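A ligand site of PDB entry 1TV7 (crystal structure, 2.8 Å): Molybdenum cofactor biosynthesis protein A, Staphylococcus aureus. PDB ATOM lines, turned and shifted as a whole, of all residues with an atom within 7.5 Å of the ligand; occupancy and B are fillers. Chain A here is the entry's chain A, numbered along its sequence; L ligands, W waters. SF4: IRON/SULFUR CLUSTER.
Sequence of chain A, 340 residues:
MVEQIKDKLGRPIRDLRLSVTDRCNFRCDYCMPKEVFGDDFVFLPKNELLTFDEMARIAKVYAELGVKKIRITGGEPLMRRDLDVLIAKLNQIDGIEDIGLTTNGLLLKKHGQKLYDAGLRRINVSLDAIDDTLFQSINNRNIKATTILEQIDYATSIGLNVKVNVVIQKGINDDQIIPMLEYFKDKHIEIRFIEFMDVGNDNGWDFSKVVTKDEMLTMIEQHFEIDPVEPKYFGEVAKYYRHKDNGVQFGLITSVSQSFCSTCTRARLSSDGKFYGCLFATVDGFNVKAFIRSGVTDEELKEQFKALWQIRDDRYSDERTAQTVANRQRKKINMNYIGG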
ATOM      1  N   THR A  21     -12.236   5.378 -13.533  1.00  0.00           N
ATOM      2  CA  THR A  21     -13.394   6.198 -13.781  1.00  0.00           C
ATOM      3  C   THR A  21     -14.164   5.764 -15.014  1.00  0.00           C
ATOM      4  O   THR A  21     -13.626   5.168 -15.919  1.00  0.00           O
ATOM      5  CB  THR A  21     -12.945   7.733 -13.953  1.00  0.00           C
ATOM      6  OG1 THR A  21     -14.099   8.606 -14.098  1.00  0.00           O
ATOM      7  CG2 THR A  21     -12.229   7.951 -15.257  1.00  0.00           C
ATOM      8  N   ASP A  22     -15.424   6.151 -15.047  1.00  0.00           N
ATOM      9  CA  ASP A  22     -16.272   5.919 -16.210  1.00  0.00           C
ATOM     10  C   ASP A  22     -16.373   7.182 -17.077  1.00  0.00           C
ATOM     11  O   ASP A  22     -16.804   7.075 -18.208  1.00  0.00           O
ATOM     12  CB  ASP A  22     -17.664   5.373 -15.782  1.00  0.00           C
ATOM     13  CG  ASP A  22     -18.421   6.316 -14.869  1.00  0.00           C
ATOM     14  OD1 ASP A  22     -17.721   7.143 -14.230  1.00  0.00           O
ATOM     15  OD2 ASP A  22     -19.699   6.311 -14.724  1.00  0.00           O
ATOM     16  N   ARG A  23     -15.967   8.334 -16.553  1.00  0.00           N
ATOM     17  CA  ARG A  23     -15.828   9.588 -17.353  1.00  0.00           C
ATOM     18  C   ARG A  23     -14.790   9.554 -18.471  1.00  0.00           C
ATOM     19  O   ARG A  23     -13.737   8.966 -18.354  1.00  0.00           O
ATOM     20  CB  ARG A  23     -15.483  10.797 -16.470  1.00  0.00           C
ATOM     21  CG  ARG A  23     -16.646  11.365 -15.779  1.00  0.00           C
ATOM     22  CD  ARG A  23     -17.294  10.463 -14.830  1.00  0.00           C
ATOM     23  NE  ARG A  23     -18.163  11.197 -13.919  1.00  0.00           N
ATOM     24  CZ  ARG A  23     -18.804  10.667 -12.877  1.00  0.00           C
ATOM     25  NH1 ARG A  23     -18.642   9.362 -12.590  1.00  0.00           N
ATOM     26  NH2 ARG A  23     -19.623  11.437 -12.119  1.00  0.00           N
ATOM     27  N   CYS A  24     -15.085  10.238 -19.558  1.00  0.00           N
ATOM     28  CA  CYS A  24     -14.062  10.583 -20.527  1.00  0.00           C
ATOM     29  C   CYS A  24     -14.183  11.969 -21.113  1.00  0.00           C
ATOM     30  O   CYS A  24     -15.278  12.509 -21.241  1.00  0.00           O
ATOM     31  CB  CYS A  24     -14.120   9.584 -21.635  1.00  0.00           C
ATOM     32  SG  CYS A  24     -12.670   9.666 -22.612  1.00  0.00           S
ATOM     33  N   ASN A  25     -13.055  12.540 -21.486  1.00  0.00           N
ATOM     34  CA  ASN A  25     -13.023  13.845 -22.179  1.00  0.00           C
ATOM     35  C   ASN A  25     -13.230  13.749 -23.713  1.00  0.00           C
ATOM     36  O   ASN A  25     -13.455  14.753 -24.371  1.00  0.00           O
ATOM     37  CB  ASN A  25     -11.784  14.709 -21.818  1.00  0.00           C
ATOM     38  CG  ASN A  25     -10.492  13.956 -21.771  1.00  0.00           C
ATOM     39  OD1 ASN A  25     -10.353  12.824 -22.206  1.00  0.00           O
ATOM     40  ND2 ASN A  25      -9.513  14.575 -21.174  1.00  0.00           N
ATOM     41  N   PHE A  26     -13.127  12.558 -24.266  1.00  0.00           N
ATOM     42  CA  PHE A  26     -13.549  12.287 -25.618  1.00  0.00           C
ATOM     43  C   PHE A  26     -14.926  11.553 -25.665  1.00  0.00           C
ATOM     44  O   PHE A  26     -15.493  11.156 -24.617  1.00  0.00           O
ATOM     45  CB  PHE A  26     -12.498  11.463 -26.337  1.00  0.00           C
ATOM     46  CG  PHE A  26     -11.155  12.157 -26.550  1.00  0.00           C
ATOM     47  CD1 PHE A  26     -10.129  11.475 -27.221  1.00  0.00           C
ATOM     48  CD2 PHE A  26     -10.903  13.458 -26.083  1.00  0.00           C
ATOM     49  CE1 PHE A  26      -8.894  12.037 -27.444  1.00  0.00           C
ATOM     50  CE2 PHE A  26      -9.673  14.043 -26.297  1.00  0.00           C
ATOM     51  CZ  PHE A  26      -8.661  13.315 -26.986  1.00  0.00           C
ATOM     52  N   ARG A  27     -15.486  11.440 -26.889  1.00  0.00           N
ATOM     53  CA  ARG A  27     -16.596  10.529 -27.213  1.00  0.00           C
ATOM     54  C   ARG A  27     -16.344   9.754 -28.500  1.00  0.00           C
ATOM     55  O   ARG A  27     -17.052   9.886 -29.476  1.00  0.00           O
ATOM     56  CB  ARG A  27     -17.885  11.323 -27.302  1.00  0.00           C
ATOM     57  CG  ARG A  27     -18.337  11.863 -25.983  1.00  0.00           C
ATOM     58  CD  ARG A  27     -18.828  10.795 -25.054  1.00  0.00           C
ATOM     59  NE  ARG A  27     -19.408  11.329 -23.829  1.00  0.00           N
ATOM     60  CZ  ARG A  27     -18.740  11.744 -22.788  1.00  0.00           C
ATOM     61  NH1 ARG A  27     -17.424  11.741 -22.760  1.00  0.00           N
ATOM     62  NH2 ARG A  27     -19.391  12.204 -21.752  1.00  0.00           N
ATOM     63  N   CYS A  28     -15.328   8.910 -28.496  1.00  0.00           N
ATOM     64  CA  CYS A  28     -14.940   8.155 -29.719  1.00  0.00           C
ATOM     65  C   CYS A  28     -15.998   7.141 -30.166  1.00  0.00           C
ATOM     66  O   CYS A  28     -16.539   6.420 -29.338  1.00  0.00           O
ATOM     67  CB  CYS A  28     -13.644   7.406 -29.438  1.00  0.00           C
ATOM     68  SG  CYS A  28     -12.408   8.433 -28.709  1.00  0.00           S
ATOM     69  N   ASP A  29     -16.280   7.079 -31.469  1.00  0.00           N
ATOM     70  CA  ASP A  29     -17.498   6.383 -31.936  1.00  0.00           C
ATOM     71  C   ASP A  29     -17.531   4.878 -31.537  1.00  0.00           C
ATOM     72  O   ASP A  29     -18.588   4.365 -31.206  1.00  0.00           O
ATOM     73  CB  ASP A  29     -17.687   6.611 -33.430  1.00  0.00           C
ATOM     74  CG  ASP A  29     -18.237   8.051 -33.749  1.00  0.00           C
ATOM     75  OD1 ASP A  29     -17.697   8.763 -34.689  1.00  0.00           O
ATOM     76  OD2 ASP A  29     -19.214   8.535 -33.107  1.00  0.00           O
ATOM     77  N   TYR A  30     -16.403   4.202 -31.497  1.00  0.00           N
ATOM     78  CA  TYR A  30     -16.385   2.763 -31.193  1.00  0.00           C
ATOM     79  C   TYR A  30     -16.313   2.426 -29.691  1.00  0.00           C
ATOM     80  O   TYR A  30     -16.262   1.267 -29.319  1.00  0.00           O
ATOM     81  CB  TYR A  30     -15.226   2.052 -31.923  1.00  0.00           C
ATOM     82  CG  TYR A  30     -13.779   2.471 -31.546  1.00  0.00           C
ATOM     83  CD1 TYR A  30     -13.053   1.779 -30.546  1.00  0.00           C
ATOM     84  CD2 TYR A  30     -13.127   3.510 -32.224  1.00  0.00           C
ATOM     85  CE1 TYR A  30     -11.733   2.146 -30.207  1.00  0.00           C
ATOM     86  CE2 TYR A  30     -11.827   3.867 -31.906  1.00  0.00           C
ATOM     87  CZ  TYR A  30     -11.134   3.187 -30.899  1.00  0.00           C
ATOM     88  OH  TYR A  30      -9.867   3.551 -30.607  1.00  0.00           O
ATOM     89  N   CYS A  31     -16.305   3.456 -28.838  1.00  0.00           N
ATOM     90  CA  CYS A  31     -16.110   3.283 -27.407  1.00  0.00           C
ATOM     91  C   CYS A  31     -17.211   3.956 -26.552  1.00  0.00           C
ATOM     92  O   CYS A  31     -17.919   3.289 -25.776  1.00  0.00           O
ATOM     93  CB  CYS A  31     -14.782   3.870 -27.035  1.00  0.00           C
ATOM     94  SG  CYS A  31     -14.530   3.765 -25.255  1.00  0.00           S
ATOM     95  N   MET A  32     -17.311   5.282 -26.688  1.00  0.00           N
ATOM     96  CA  MET A  32     -18.347   6.067 -26.019  1.00  0.00           C
ATOM     97  C   MET A  32     -19.072   6.978 -27.023  1.00  0.00           C
ATOM     98  O   MET A  32     -19.047   8.170 -26.862  1.00  0.00           O
ATOM     99  CB  MET A  32     -17.727   6.900 -24.899  1.00  0.00           C
ATOM    100  CG  MET A  32     -16.960   6.121 -23.872  1.00  0.00           C
ATOM    101  SD  MET A  32     -16.264   7.114 -22.512  1.00  0.00           S
ATOM    102  CE  MET A  32     -17.669   7.536 -21.519  1.00  0.00           C
ATOM    103  N   PRO A  33     -19.766   6.430 -28.014  1.00  0.00           N
ATOM    104  CA  PRO A  33     -20.434   7.260 -29.048  1.00  0.00           C
ATOM    105  C   PRO A  33     -21.403   8.273 -28.441  1.00  0.00           C
ATOM    106  O   PRO A  33     -22.099   7.866 -27.519  1.00  0.00           O
ATOM    107  CB  PRO A  33     -21.186   6.243 -29.938  1.00  0.00           C
ATOM    108  CG  PRO A  33     -21.302   5.004 -29.094  1.00  0.00           C
ATOM    109  CD  PRO A  33     -20.035   4.988 -28.196  1.00  0.00           C
ATOM    110  N   PHE A  37     -23.770   8.101 -24.802  1.00  0.00           N
ATOM    111  CA  PHE A  37     -23.287   8.958 -23.701  1.00  0.00           C
ATOM    112  C   PHE A  37     -23.458  10.451 -24.031  1.00  0.00           C
ATOM    113  O   PHE A  37     -22.497  11.199 -24.056  1.00  0.00           O
ATOM    114  CB  PHE A  37     -21.835   8.661 -23.410  1.00  0.00           C
ATOM    115  CG  PHE A  37     -21.540   7.228 -23.076  1.00  0.00           C
ATOM    116  CD1 PHE A  37     -21.306   6.303 -24.089  1.00  0.00           C
ATOM    117  CD2 PHE A  37     -21.436   6.809 -21.761  1.00  0.00           C
ATOM    118  CE1 PHE A  37     -21.011   4.964 -23.785  1.00  0.00           C
ATOM    119  CE2 PHE A  37     -21.138   5.476 -21.434  1.00  0.00           C
ATOM    120  CZ  PHE A  37     -20.907   4.554 -22.459  1.00  0.00           C
ATOM    121  N   GLY A  74      -9.572   4.015 -17.700  1.00  0.00           N
ATOM    122  CA  GLY A  74     -10.876   4.582 -17.362  1.00  0.00           C
ATOM    123  C   GLY A  74     -11.930   4.085 -18.298  1.00  0.00           C
ATOM    124  O   GLY A  74     -12.012   2.949 -18.461  1.00  0.00           O
ATOM    125  N   GLY A  75     -12.677   4.913 -18.972  1.00  0.00           N
ATOM    126  CA  GLY A  75     -12.544   6.335 -18.909  1.00  0.00           C
ATOM    127  C   GLY A  75     -11.224   6.864 -19.382  1.00  0.00           C
ATOM    128  O   GLY A  75     -10.402   6.124 -19.928  1.00  0.00           O
ATOM    129  N   GLU A  76     -11.058   8.152 -19.164  1.00  0.00           N
ATOM    130  CA  GLU A  76      -9.792   8.792 -19.238  1.00  0.00           C
ATOM    131  C   GLU A  76      -9.354   8.892 -17.785  1.00  0.00           C
ATOM    132  O   GLU A  76      -9.978   9.605 -17.015  1.00  0.00           O
ATOM    133  CB  GLU A  76      -9.963  10.197 -19.824  1.00  0.00           C
ATOM    134  CG  GLU A  76      -8.723  11.054 -19.739  1.00  0.00           C
ATOM    135  CD  GLU A  76      -7.493  10.273 -20.064  1.00  0.00           C
ATOM    136  OE1 GLU A  76      -6.549  10.450 -19.332  1.00  0.00           O
ATOM    137  OE2 GLU A  76      -7.491   9.482 -21.026  1.00  0.00           O
ATOM    138  N   PRO A  77      -8.306   8.173 -17.398  1.00  0.00           N
ATOM    139  CA  PRO A  77      -7.901   8.133 -15.997  1.00  0.00           C
ATOM    140  C   PRO A  77      -7.567   9.474 -15.401  1.00  0.00           C
ATOM    141  O   PRO A  77      -7.835   9.689 -14.228  1.00  0.00           O
ATOM    142  CB  PRO A  77      -6.622   7.282 -16.025  1.00  0.00           C
ATOM    143  CG  PRO A  77      -6.709   6.550 -17.313  1.00  0.00           C
ATOM    144  CD  PRO A  77      -7.437   7.353 -18.266  1.00  0.00           C
ATOM    145  N   THR A 102      -2.919   4.022 -19.294  1.00  0.00           N
ATOM    146  CA  THR A 102      -3.302   4.453 -20.617  1.00  0.00           C
ATOM    147  C   THR A 102      -4.303   5.558 -20.640  1.00  0.00           C
ATOM    148  O   THR A 102      -5.299   5.547 -19.956  1.00  0.00           O
ATOM    149  CB  THR A 102      -3.589   3.283 -21.638  1.00  0.00           C
ATOM    150  OG1 THR A 102      -4.934   3.328 -22.118  1.00  0.00           O
ATOM    151  CG2 THR A 102      -3.436   1.976 -21.068  1.00  0.00           C
ATOM    152  N   THR A 103      -4.023   6.497 -21.505  1.00  0.00           N
ATOM    153  CA  THR A 103      -4.714   7.771 -21.554  1.00  0.00           C
ATOM    154  C   THR A 103      -4.678   8.257 -22.978  1.00  0.00           C
ATOM    155  O   THR A 103      -3.754   7.901 -23.763  1.00  0.00           O
ATOM    156  CB  THR A 103      -3.931   8.732 -20.663  1.00  0.00           C
ATOM    157  OG1 THR A 103      -4.389  10.042 -20.845  1.00  0.00           O
ATOM    158  CG2 THR A 103      -2.494   8.836 -21.105  1.00  0.00           C
ATOM    159  N   ASN A 104      -5.658   9.069 -23.309  1.00  0.00           N
ATOM    160  CA  ASN A 104      -5.623   9.827 -24.570  1.00  0.00           C
ATOM    161  C   ASN A 104      -4.620  10.965 -24.454  1.00  0.00           C
ATOM    162  O   ASN A 104      -4.382  11.661 -25.380  1.00  0.00           O
ATOM    163  CB  ASN A 104      -7.003  10.339 -24.920  1.00  0.00           C
ATOM    164  CG  ASN A 104      -7.559  11.292 -23.857  1.00  0.00           C
ATOM    165  OD1 ASN A 104      -6.813  12.099 -23.208  1.00  0.00           O
ATOM    166  ND2 ASN A 104      -8.837  11.184 -23.638  1.00  0.00           N
ATOM    167  N   GLY A 105      -4.096  11.211 -23.275  1.00  0.00           N
ATOM    168  CA  GLY A 105      -3.003  12.176 -23.122  1.00  0.00           C
ATOM    169  C   GLY A 105      -3.380  13.632 -23.008  1.00  0.00           C
ATOM    170  O   GLY A 105      -2.534  14.470 -22.786  1.00  0.00           O
ATOM    171  N   SER A 126      -3.226   6.643 -26.371  1.00  0.00           N
ATOM    172  CA  SER A 126      -4.110   6.305 -27.488  1.00  0.00           C
ATOM    173  C   SER A 126      -4.274   7.466 -28.432  1.00  0.00           C
ATOM    174  O   SER A 126      -4.878   8.452 -28.052  1.00  0.00           O
ATOM    175  CB  SER A 126      -5.467   5.998 -26.959  1.00  0.00           C
ATOM    176  OG  SER A 126      -5.393   4.887 -26.188  1.00  0.00           O
ATOM    177  N   ASP A 128      -5.505   7.804 -32.502  1.00  0.00           N
ATOM    178  CA  ASP A 128      -5.955   7.043 -33.652  1.00  0.00           C
ATOM    179  C   ASP A 128      -5.683   7.676 -35.016  1.00  0.00           C
ATOM    180  O   ASP A 128      -5.930   7.041 -36.056  1.00  0.00           O
ATOM    181  CB  ASP A 128      -7.422   6.678 -33.474  1.00  0.00           C
ATOM    182  CG  ASP A 128      -7.612   5.431 -32.610  1.00  0.00           C
ATOM    183  OD1 ASP A 128      -6.619   4.753 -32.269  1.00  0.00           O
ATOM    184  OD2 ASP A 128      -8.730   5.048 -32.215  1.00  0.00           O
ATOM    185  N   ILE A 138     -12.844  11.566 -35.133  1.00  0.00           N
ATOM    186  CA  ILE A 138     -12.801  10.399 -34.301  1.00  0.00           C
ATOM    187  C   ILE A 138     -13.134  10.702 -32.858  1.00  0.00           C
ATOM    188  O   ILE A 138     -13.950   9.991 -32.289  1.00  0.00           O
ATOM    189  CB  ILE A 138     -11.404   9.661 -34.415  1.00  0.00           C
ATOM    190  CG1 ILE A 138     -11.206   9.139 -35.818  1.00  0.00           C
ATOM    191  CG2 ILE A 138     -11.308   8.469 -33.459  1.00  0.00           C
ATOM    192  CD1 ILE A 138      -9.784   8.713 -36.053  1.00  0.00           C
ATOM    193  N   ASN A 139     -12.525  11.713 -32.244  1.00  0.00           N
ATOM    194  CA  ASN A 139     -12.777  11.941 -30.799  1.00  0.00           C
ATOM    195  C   ASN A 139     -14.158  12.647 -30.513  1.00  0.00           C
ATOM    196  O   ASN A 139     -14.766  12.459 -29.445  1.00  0.00           O
ATOM    197  CB  ASN A 139     -11.594  12.675 -30.136  1.00  0.00           C
ATOM    198  CG  ASN A 139     -11.382  14.110 -30.687  1.00  0.00           C
ATOM    199  OD1 ASN A 139     -12.303  14.927 -30.637  1.00  0.00           O
ATOM    200  ND2 ASN A 139     -10.180  14.408 -31.200  1.00  0.00           N
ATOM    201  N   VAL A 167      -5.536   2.153 -32.973  1.00  0.00           N
ATOM    202  CA  VAL A 167      -6.536   1.227 -33.479  1.00  0.00           C
ATOM    203  C   VAL A 167      -6.892   1.651 -34.922  1.00  0.00           C
ATOM    204  O   VAL A 167      -7.404   2.753 -35.158  1.00  0.00           O
ATOM    205  CB  VAL A 167      -7.817   1.303 -32.627  1.00  0.00           C
ATOM    206  CG1 VAL A 167      -8.877   0.352 -33.162  1.00  0.00           C
ATOM    207  CG2 VAL A 167      -7.540   0.978 -31.196  1.00  0.00           C
HETATM  208 FE1  SF4 L   1     -12.495   7.960 -24.064  1.00  0.00          FE
HETATM  209 FE2  SF4 L   1     -13.046   5.571 -25.092  1.00  0.00          FE
HETATM  210 FE3  SF4 L   1     -12.172   7.457 -26.711  1.00  0.00          FE
HETATM  211 FE4  SF4 L   1     -10.556   6.111 -24.877  1.00  0.00          FE
HETATM  212  S1  SF4 L   1     -11.512   5.276 -26.716  1.00  0.00           S
HETATM  213  S2  SF4 L   1     -10.639   8.331 -25.341  1.00  0.00           S
HETATM  214  S3  SF4 L   1     -12.041   5.915 -23.146  1.00  0.00           S
HETATM  215  S4  SF4 L   1     -14.167   7.510 -25.629  1.00  0.00           S
HETATM  216  O   HOH W   1      -8.184   5.442 -24.368  1.00  0.00           O
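The backbone NH of Cys 28 sits close to a sulfur (S4) of the ligand, 3.4 Å away.
FE3 of the ligand is bound by SG of Cys 28 (2.2 Å).
The side-chain sulfur (SG) of Cys 24 is bound to an iron atom (FE1) of the ligand, at 2.2 Å.
SG of Cys 31 binds FE2 of the ligand, 2.3 Å away.
ND2 of Asn 104 lies close to S2 of the ligand (3.8 Å).
The backbone NH (N) of Phe 26 lies close to the side-chain sulfur (SG) of Cys 24, at 3.4 Å.
The guanidinium group (NH1) of Arg 27 lies within hydrogen-bond range of the backbone carbonyl oxygen (O) of Cys 24.
N of Gly 75 sits at hydrogen-bond distance from O of Thr 21 (3.2 Å).
OE2 of Glu 76 sits at hydrogen-bond distance from N of Asn 104.
ND2 of Asn 104 lies within hydrogen-bond range of OD1 of Asn 25 (2.7 Å).
A sulfur (S4) of the ligand sits close to the side-chain sulfur (SD) of Met 32, at 3.8 Å.
The backbone carbonyl oxygen (O) of Gly 75 sits close to a sulfur (S3) of the ligand, 3.6 Å away.
CD1 of Phe 26 touches S2 of the ligand, at 3.7 Å.
Seven residues have an atom within 4 Å of the ligand: Cys 24, Phe 26, Cys 28, Cys 31, Met 32, Gly 75 and Asn 104.
The nearest printed residue that does not touch the ligand is Arg 27 (4.2 Å).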
